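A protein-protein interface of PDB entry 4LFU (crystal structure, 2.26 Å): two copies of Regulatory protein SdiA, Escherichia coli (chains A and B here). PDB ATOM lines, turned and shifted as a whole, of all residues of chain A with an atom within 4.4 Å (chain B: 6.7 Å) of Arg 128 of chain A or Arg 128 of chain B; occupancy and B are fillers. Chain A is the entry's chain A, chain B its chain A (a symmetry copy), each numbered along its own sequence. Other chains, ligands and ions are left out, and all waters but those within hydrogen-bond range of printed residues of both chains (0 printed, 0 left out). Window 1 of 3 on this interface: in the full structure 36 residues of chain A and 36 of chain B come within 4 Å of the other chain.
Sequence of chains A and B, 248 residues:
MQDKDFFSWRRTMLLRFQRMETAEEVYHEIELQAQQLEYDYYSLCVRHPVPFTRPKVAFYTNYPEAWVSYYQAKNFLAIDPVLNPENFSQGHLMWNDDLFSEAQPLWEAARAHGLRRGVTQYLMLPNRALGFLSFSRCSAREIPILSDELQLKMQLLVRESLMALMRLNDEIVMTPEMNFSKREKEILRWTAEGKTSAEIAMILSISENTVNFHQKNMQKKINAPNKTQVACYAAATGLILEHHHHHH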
ATOM      1  N   PRO A  49      -5.276  15.125 -13.237  1.00  0.00           N
ATOM      2  CA  PRO A  49      -5.541  13.695 -13.188  1.00  0.00           C
ATOM      3  C   PRO A  49      -4.732  12.987 -12.087  1.00  0.00           C
ATOM      4  O   PRO A  49      -5.115  11.910 -11.651  1.00  0.00           O
ATOM      5  CB  PRO A  49      -5.096  13.222 -14.566  1.00  0.00           C
ATOM      6  CG  PRO A  49      -4.003  14.137 -14.914  1.00  0.00           C
ATOM      7  CD  PRO A  49      -4.522  15.489 -14.448  1.00  0.00           C
ATOM      8  N   MET A 124     -12.432  18.812 -20.604  1.00  0.00           N
ATOM      9  CA  MET A 124     -11.306  17.931 -20.346  1.00  0.00           C
ATOM     10  C   MET A 124     -10.190  18.241 -21.315  1.00  0.00           C
ATOM     11  O   MET A 124     -10.396  18.235 -22.517  1.00  0.00           O
ATOM     12  CB  MET A 124     -11.678  16.463 -20.502  1.00  0.00           C
ATOM     13  CG  MET A 124     -10.431  15.582 -20.385  1.00  0.00           C
ATOM     14  SD  MET A 124     -10.848  13.880 -20.077  1.00  0.00           S
ATOM     15  CE  MET A 124     -11.534  13.371 -21.661  1.00  0.00           C
ATOM     16  N   LEU A 125      -8.997  18.479 -20.780  1.00  0.00           N
ATOM     17  CA  LEU A 125      -7.816  18.797 -21.606  1.00  0.00           C
ATOM     18  C   LEU A 125      -7.090  17.554 -22.185  1.00  0.00           C
ATOM     19  O   LEU A 125      -7.313  16.426 -21.714  1.00  0.00           O
ATOM     20  CB  LEU A 125      -6.864  19.704 -20.816  1.00  0.00           C
ATOM     21  CG  LEU A 125      -7.557  20.972 -20.305  1.00  0.00           C
ATOM     22  CD1 LEU A 125      -6.767  21.591 -19.167  1.00  0.00           C
ATOM     23  CD2 LEU A 125      -7.799  21.965 -21.433  1.00  0.00           C
ATOM     24  N   PRO A 126      -6.201  17.759 -23.191  1.00  0.00           N
ATOM     25  CA  PRO A 126      -5.473  16.598 -23.784  1.00  0.00           C
ATOM     26  C   PRO A 126      -4.686  15.790 -22.743  1.00  0.00           C
ATOM     27  O   PRO A 126      -4.444  14.604 -22.947  1.00  0.00           O
ATOM     28  CB  PRO A 126      -4.521  17.242 -24.812  1.00  0.00           C
ATOM     29  CG  PRO A 126      -5.158  18.628 -25.111  1.00  0.00           C
ATOM     30  CD  PRO A 126      -5.807  19.045 -23.814  1.00  0.00           C
ATOM     31  N   ASN A 127      -4.323  16.424 -21.627  1.00  0.00           N
ATOM     32  CA  ASN A 127      -3.587  15.753 -20.554  1.00  0.00           C
ATOM     33  C   ASN A 127      -4.500  15.132 -19.481  1.00  0.00           C
ATOM     34  O   ASN A 127      -4.024  14.570 -18.474  1.00  0.00           O
ATOM     35  CB  ASN A 127      -2.555  16.702 -19.934  1.00  0.00           C
ATOM     36  CG  ASN A 127      -3.187  17.907 -19.218  1.00  0.00           C
ATOM     37  OD1 ASN A 127      -4.409  18.062 -19.164  1.00  0.00           O
ATOM     38  ND2 ASN A 127      -2.336  18.763 -18.659  1.00  0.00           N
ATOM     39  N   ARG A 128      -5.816  15.219 -19.737  1.00  0.00           N
ATOM     40  CA  ARG A 128      -6.880  14.665 -18.869  1.00  0.00           C
ATOM     41  C   ARG A 128      -7.147  15.509 -17.610  1.00  0.00           C
ATOM     42  O   ARG A 128      -7.887  15.096 -16.717  1.00  0.00           O
ATOM     43  CB  ARG A 128      -6.595  13.213 -18.497  1.00  0.00           C
ATOM     44  CG  ARG A 128      -6.815  12.224 -19.601  1.00  0.00           C
ATOM     45  CD  ARG A 128      -5.692  12.245 -20.622  1.00  0.00           C
ATOM     46  NE  ARG A 128      -5.625  10.973 -21.330  1.00  0.00           N
ATOM     47  CZ  ARG A 128      -5.441  10.860 -22.634  1.00  0.00           C
ATOM     48  NH1 ARG A 128      -5.244  11.951 -23.366  1.00  0.00           N
ATOM     49  NH2 ARG A 128      -5.415   9.658 -23.190  1.00  0.00           N
ATOM     50  N   ALA A 129      -6.544  16.690 -17.534  1.00  0.00           N
ATOM     51  CA  ALA A 129      -6.917  17.638 -16.488  1.00  0.00           C
ATOM     52  C   ALA A 129      -8.317  18.110 -16.815  1.00  0.00           C
ATOM     53  O   ALA A 129      -8.710  18.138 -17.981  1.00  0.00           O
ATOM     54  CB  ALA A 129      -5.947  18.810 -16.445  1.00  0.00           C
ATOM     55  N   LEU A 130      -9.080  18.477 -15.794  1.00  0.00           N
ATOM     56  CA  LEU A 130     -10.416  19.008 -16.033  1.00  0.00           C
ATOM     57  C   LEU A 130     -10.396  20.479 -15.692  1.00  0.00           C
ATOM     58  O   LEU A 130     -10.081  20.860 -14.552  1.00  0.00           O
ATOM     59  CB  LEU A 130     -11.470  18.265 -15.187  1.00  0.00           C
ATOM     60  CG  LEU A 130     -11.765  16.778 -15.431  1.00  0.00           C
ATOM     61  CD1 LEU A 130     -12.804  16.336 -14.426  1.00  0.00           C
ATOM     62  CD2 LEU A 130     -12.303  16.529 -16.841  1.00  0.00           C
ATOM     63  N   ALA A 236      -2.592   7.620 -17.295  1.00  0.00           N
ATOM     64  CA  ALA A 236      -3.585   8.644 -16.902  1.00  0.00           C
ATOM     65  C   ALA A 236      -3.497   9.941 -17.701  1.00  0.00           C
ATOM     66  O   ALA A 236      -4.526  10.546 -18.036  1.00  0.00           O
ATOM     67  CB  ALA A 236      -3.497   8.934 -15.432  1.00  0.00           C
ATOM     68  N   THR A 237      -2.260  10.380 -17.969  1.00  0.00           N
ATOM     69  CA  THR A 237      -2.009  11.646 -18.638  1.00  0.00           C
ATOM     70  C   THR A 237      -1.959  11.500 -20.154  1.00  0.00           C
ATOM     71  O   THR A 237      -1.889  12.495 -20.871  1.00  0.00           O
ATOM     72  CB  THR A 237      -0.689  12.263 -18.175  1.00  0.00           C
ATOM     73  OG1 THR A 237       0.345  11.293 -18.366  1.00  0.00           O
ATOM     74  CG2 THR A 237      -0.753  12.654 -16.713  1.00  0.00           C
ATOM     75  N   GLY A 238      -1.951  10.261 -20.630  1.00  0.00           N
ATOM     76  CA  GLY A 238      -1.955   9.976 -22.053  1.00  0.00           C
ATOM     77  C   GLY A 238      -0.581   9.958 -22.683  1.00  0.00           C
ATOM     78  O   GLY A 238      -0.477  10.023 -23.897  1.00  0.00           O
ATOM     79  N   ARG B  47     -10.386   5.426 -32.216  1.00  0.00           N
ATOM     80  CA  ARG B  47      -9.181   4.819 -31.651  1.00  0.00           C
ATOM     81  C   ARG B  47      -9.376   4.702 -30.135  1.00  0.00           C
ATOM     82  O   ARG B  47      -9.389   5.700 -29.415  1.00  0.00           O
ATOM     83  CB  ARG B  47      -7.865   5.632 -31.953  1.00  0.00           C
ATOM     84  CG  ARG B  47      -7.801   6.402 -33.310  1.00  0.00           C
ATOM     85  CD  ARG B  47      -6.352   6.911 -33.731  1.00  0.00           C
ATOM     86  NE  ARG B  47      -5.523   5.752 -34.075  1.00  0.00           N
ATOM     87  CZ  ARG B  47      -4.656   5.663 -35.084  1.00  0.00           C
ATOM     88  NH1 ARG B  47      -4.441   6.682 -35.911  1.00  0.00           N
ATOM     89  NH2 ARG B  47      -3.994   4.522 -35.262  1.00  0.00           N
ATOM     90  N   HIS B  48      -9.552   3.469 -29.677  1.00  0.00           N
ATOM     91  CA  HIS B  48      -9.731   3.176 -28.265  1.00  0.00           C
ATOM     92  C   HIS B  48      -8.427   3.349 -27.478  1.00  0.00           C
ATOM     93  O   HIS B  48      -7.340   3.145 -28.023  1.00  0.00           O
ATOM     94  CB  HIS B  48     -10.291   1.768 -28.095  1.00  0.00           C
ATOM     95  CG  HIS B  48     -11.725   1.646 -28.509  1.00  0.00           C
ATOM     96  ND1 HIS B  48     -12.153   1.897 -29.798  1.00  0.00           N
ATOM     97  CD2 HIS B  48     -12.829   1.290 -27.809  1.00  0.00           C
ATOM     98  CE1 HIS B  48     -13.457   1.705 -29.873  1.00  0.00           C
ATOM     99  NE2 HIS B  48     -13.891   1.333 -28.681  1.00  0.00           N
ATOM    100  N   PRO B  49      -8.530   3.744 -26.196  1.00  0.00           N
ATOM    101  CA  PRO B  49      -7.335   3.931 -25.386  1.00  0.00           C
ATOM    102  C   PRO B  49      -6.622   2.602 -25.080  1.00  0.00           C
ATOM    103  O   PRO B  49      -5.437   2.606 -24.776  1.00  0.00           O
ATOM    104  CB  PRO B  49      -7.887   4.547 -24.107  1.00  0.00           C
ATOM    105  CG  PRO B  49      -9.229   3.964 -23.988  1.00  0.00           C
ATOM    106  CD  PRO B  49      -9.751   4.005 -25.417  1.00  0.00           C
ATOM    107  N   MET B 124     -11.747  13.933 -28.411  1.00  0.00           N
ATOM    108  CA  MET B 124     -11.477  12.947 -27.379  1.00  0.00           C
ATOM    109  C   MET B 124     -12.699  12.779 -26.508  1.00  0.00           C
ATOM    110  O   MET B 124     -13.211  13.746 -25.971  1.00  0.00           O
ATOM    111  CB  MET B 124     -10.310  13.351 -26.489  1.00  0.00           C
ATOM    112  CG  MET B 124     -10.166  12.372 -25.321  1.00  0.00           C
ATOM    113  SD  MET B 124      -8.571  12.499 -24.541  1.00  0.00           S
ATOM    114  CE  MET B 124      -8.692  14.086 -23.702  1.00  0.00           C
ATOM    115  N   LEU B 125     -13.141  11.535 -26.349  1.00  0.00           N
ATOM    116  CA  LEU B 125     -14.326  11.223 -25.527  1.00  0.00           C
ATOM    117  C   LEU B 125     -14.034  11.105 -24.008  1.00  0.00           C
ATOM    118  O   LEU B 125     -12.866  10.969 -23.606  1.00  0.00           O
ATOM    119  CB  LEU B 125     -15.021   9.973 -26.080  1.00  0.00           C
ATOM    120  CG  LEU B 125     -15.380  10.112 -27.563  1.00  0.00           C
ATOM    121  CD1 LEU B 125     -15.614   8.749 -28.187  1.00  0.00           C
ATOM    122  CD2 LEU B 125     -16.572  11.038 -27.760  1.00  0.00           C
ATOM    123  N   PRO B 126     -15.096  11.130 -23.161  1.00  0.00           N
ATOM    124  CA  PRO B 126     -14.871  11.019 -21.689  1.00  0.00           C
ATOM    125  C   PRO B 126     -14.106   9.748 -21.296  1.00  0.00           C
ATOM    126  O   PRO B 126     -13.447   9.729 -20.259  1.00  0.00           O
ATOM    127  CB  PRO B 126     -16.295  11.005 -21.097  1.00  0.00           C
ATOM    128  CG  PRO B 126     -17.178  11.651 -22.202  1.00  0.00           C
ATOM    129  CD  PRO B 126     -16.533  11.242 -23.503  1.00  0.00           C
ATOM    130  N   ASN B 127     -14.169   8.714 -22.134  1.00  0.00           N
ATOM    131  CA  ASN B 127     -13.464   7.456 -21.876  1.00  0.00           C
ATOM    132  C   ASN B 127     -12.051   7.410 -22.488  1.00  0.00           C
ATOM    133  O   ASN B 127     -11.343   6.387 -22.400  1.00  0.00           O
ATOM    134  CB  ASN B 127     -14.312   6.262 -22.326  1.00  0.00           C
ATOM    135  CG  ASN B 127     -14.548   6.219 -23.845  1.00  0.00           C
ATOM    136  OD1 ASN B 127     -14.084   7.077 -24.599  1.00  0.00           O
ATOM    137  ND2 ASN B 127     -15.277   5.199 -24.291  1.00  0.00           N
ATOM    138  N   ARG B 128     -11.652   8.549 -23.079  1.00  0.00           N
ATOM    139  CA  ARG B 128     -10.325   8.752 -23.703  1.00  0.00           C
ATOM    140  C   ARG B 128     -10.186   8.078 -25.081  1.00  0.00           C
ATOM    141  O   ARG B 128      -9.097   8.023 -25.651  1.00  0.00           O
ATOM    142  CB  ARG B 128      -9.199   8.315 -22.772  1.00  0.00           C
ATOM    143  CG  ARG B 128      -8.933   9.243 -21.625  1.00  0.00           C
ATOM    144  CD  ARG B 128      -9.972   9.110 -20.527  1.00  0.00           C
ATOM    145  NE  ARG B 128      -9.427   9.563 -19.254  1.00  0.00           N
ATOM    146  CZ  ARG B 128     -10.089  10.315 -18.391  1.00  0.00           C
ATOM    147  NH1 ARG B 128     -11.350  10.648 -18.643  1.00  0.00           N
ATOM    148  NH2 ARG B 128      -9.500  10.694 -17.267  1.00  0.00           N
ATOM    149  N   ALA B 129     -11.287   7.563 -25.617  1.00  0.00           N
ATOM    150  CA  ALA B 129     -11.284   7.111 -27.004  1.00  0.00           C
ATOM    151  C   ALA B 129     -11.165   8.352 -27.862  1.00  0.00           C
ATOM    152  O   ALA B 129     -11.600   9.432 -27.460  1.00  0.00           O
ATOM    153  CB  ALA B 129     -12.561   6.349 -27.331  1.00  0.00           C
ATOM    154  N   LEU B 130     -10.573   8.214 -29.040  1.00  0.00           N
ATOM    155  CA  LEU B 130     -10.482   9.348 -29.951  1.00  0.00           C
ATOM    156  C   LEU B 130     -11.398   9.076 -31.120  1.00  0.00           C
ATOM    157  O   LEU B 130     -11.241   8.065 -31.824  1.00  0.00           O
ATOM    158  CB  LEU B 130      -9.032   9.561 -30.431  1.00  0.00           C
ATOM    159  CG  LEU B 130      -7.931   9.969 -29.442  1.00  0.00           C
ATOM    160  CD1 LEU B 130      -6.627  10.058 -30.203  1.00  0.00           C
ATOM    161  CD2 LEU B 130      -8.220  11.325 -28.797  1.00  0.00           C
ATOM    162  N   THR B 175     -15.362   1.122 -24.101  1.00  0.00           N
ATOM    163  CA  THR B 175     -14.125   0.514 -23.598  1.00  0.00           C
ATOM    164  C   THR B 175     -14.515  -0.649 -22.666  1.00  0.00           C
ATOM    165  O   THR B 175     -15.683  -0.754 -22.314  1.00  0.00           O
ATOM    166  CB  THR B 175     -13.220   1.578 -22.899  1.00  0.00           C
ATOM    167  OG1 THR B 175     -14.010   2.402 -22.018  1.00  0.00           O
ATOM    168  CG2 THR B 175     -12.581   2.472 -23.934  1.00  0.00           C
ATOM    169  N   ALA B 234      -7.861   1.080 -15.736  1.00  0.00           N
ATOM    170  CA  ALA B 234      -8.631   2.050 -14.944  1.00  0.00           C
ATOM    171  C   ALA B 234      -8.152   3.506 -15.086  1.00  0.00           C
ATOM    172  O   ALA B 234      -8.947   4.437 -15.269  1.00  0.00           O
ATOM    173  CB  ALA B 234      -8.564   1.640 -13.485  1.00  0.00           C
ATOM    174  N   ALA B 235      -6.840   3.690 -14.961  1.00  0.00           N
ATOM    175  CA  ALA B 235      -6.209   4.984 -15.136  1.00  0.00           C
ATOM    176  C   ALA B 235      -6.439   5.523 -16.565  1.00  0.00           C
ATOM    177  O   ALA B 235      -6.802   6.701 -16.730  1.00  0.00           O
ATOM    178  CB  ALA B 235      -4.761   4.884 -14.832  1.00  0.00           C
ATOM    179  N   ALA B 236      -6.286   4.657 -17.586  1.00  0.00           N
ATOM    180  CA  ALA B 236      -6.391   5.102 -18.993  1.00  0.00           C
ATOM    181  C   ALA B 236      -7.789   5.557 -19.403  1.00  0.00           C
ATOM    182  O   ALA B 236      -7.938   6.529 -20.158  1.00  0.00           O
ATOM    183  CB  ALA B 236      -5.899   4.035 -19.926  1.00  0.00           C
ATOM    184  N   THR B 237      -8.805   4.822 -18.931  1.00  0.00           N
ATOM    185  CA  THR B 237     -10.187   5.070 -19.308  1.00  0.00           C
ATOM    186  C   THR B 237     -10.872   6.064 -18.378  1.00  0.00           C
ATOM    187  O   THR B 237     -11.997   6.482 -18.636  1.00  0.00           O
ATOM    188  CB  THR B 237     -11.002   3.776 -19.303  1.00  0.00           C
ATOM    189  OG1 THR B 237     -10.852   3.162 -18.019  1.00  0.00           O
ATOM    190  CG2 THR B 237     -10.518   2.824 -20.378  1.00  0.00           C
ATOM    191  N   GLY B 238     -10.207   6.403 -17.280  1.00  0.00           N
ATOM    192  CA  GLY B 238     -10.717   7.376 -16.332  1.00  0.00           C
ATOM    193  C   GLY B 238     -11.642   6.795 -15.288  1.00  0.00           C
ATOM    194  O   GLY B 238     -12.354   7.541 -14.635  1.00  0.00           O
ATOM    195  N   LEU B 239     -11.649   5.471 -15.128  1.00  0.00           N
ATOM    196  CA  LEU B 239     -12.499   4.830 -14.103  1.00  0.00           C
ATOM    197  C   LEU B 239     -12.034   5.226 -12.699  1.00  0.00           C
ATOM    198  O   LEU B 239     -12.854   5.529 -11.823  1.00  0.00           O
ATOM    199  CB  LEU B 239     -12.505   3.307 -14.240  1.00  0.00           C
ATOM    200  CG  LEU B 239     -12.983   2.528 -13.003  1.00  0.00           C
ATOM    201  CD1 LEU B 239     -14.494   2.303 -13.022  1.00  0.00           C
ATOM    202  CD2 LEU B 239     -12.242   1.196 -12.836  1.00  0.00           C
ATOM    203  N   ILE B 240     -10.710   5.205 -12.525  1.00  0.00           N
ATOM    204  CA  ILE B 240      -9.972   5.660 -11.351  1.00  0.00           C
ATOM    205  C   ILE B 240     -10.202   7.163 -11.073  1.00  0.00           C
ATOM    206  O   ILE B 240     -10.563   7.964 -11.957  1.00  0.00           O
ATOM    207  CB  ILE B 240      -8.441   5.376 -11.599  1.00  0.00           C
ATOM    208  CG1 ILE B 240      -7.928   4.210 -10.746  1.00  0.00           C
ATOM    209  CG2 ILE B 240      -7.603   6.606 -11.369  1.00  0.00           C
ATOM    210  CD1 ILE B 240      -6.429   3.966 -10.889  1.00  0.00           C
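Met 124 of chain A touches its own counterpart, Met 124 of chain B.
Met 124 of chain A touches Leu 125 of chain B, and with the chains exchanged Leu 125 of chain A touches Met 124 of chain B.
Met 124 of chain A touches Arg 128 of chain B, and with the chains exchanged Arg 128 of chain A touches Met 124 of chain B.
Arg 128 of chain B touches its own counterpart, Arg 128 of chain A.
The guanidinium group of Arg 128 of chain B lies close to the backbone carbonyl oxygen of Ala 236 of chain B, 3.5 Å away.
O of Ala 236 of chain A lies close to NE of Arg 128 of chain A (3.5 Å).
O of Pro 126 of chain A lies within hydrogen-bond range of NH1 of Arg 128 of chain A, 2.8 Å away.
NH1 of Arg 128 of chain B sits at hydrogen-bond distance from O of Pro 126 of chain B.
Met 124 of chain A touches Met 124 of chain B.
Met 124 of chain A touches Leu 125 of chain B.
Met 124 of chain B touches Leu 125 of chain A.
Arg 128 of chain B touches Arg 128 of chain A.
CA of Ala 236 of chain A touches O of Ala 235 of chain B (3.8 Å).
Of the 11 printed residues of chain A, 4 touch a printed residue of chain B.
Along chain A the printed residues that touch a printed residue of chain B span positions 124 to 236.
Along chain B the printed residues that touch a printed residue of chain A span positions 124 to 235.
Among the printed residues, no Asp or Glu carboxylate lies within 4 Å of a Lys or Arg side-chain nitrogen of the other chain.
Of the printed residues of chain B, Met 124 of chain A touches Met 124, Leu 125 and Arg 128.
Arg 128 of chain A touches just these residues of chain B: Met 124 (3.6 Å) and Arg 128 (3.7 Å).
Of the printed residues of chain A, Leu 125 of chain B touches Met 124 (3.4 Å).
The nearest residue of chain B that does not touch Arg 128 of chain A is Ala 236 of chain B (5.0 Å).
The nearest printed residue of chain A that does not touch Arg 128 of chain B is Ala 236 of chain A (5.0 Å).
NH1 of Arg 128 of chain A sits at hydrogen-bond distance from SD of Met 124 of chain B.
The guanidinium group (NH1) of Arg 128 of chain B is in hydrogen-bond range of the side-chain sulfur (SD) of Met 124 of chain A, 3.6 Å away.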
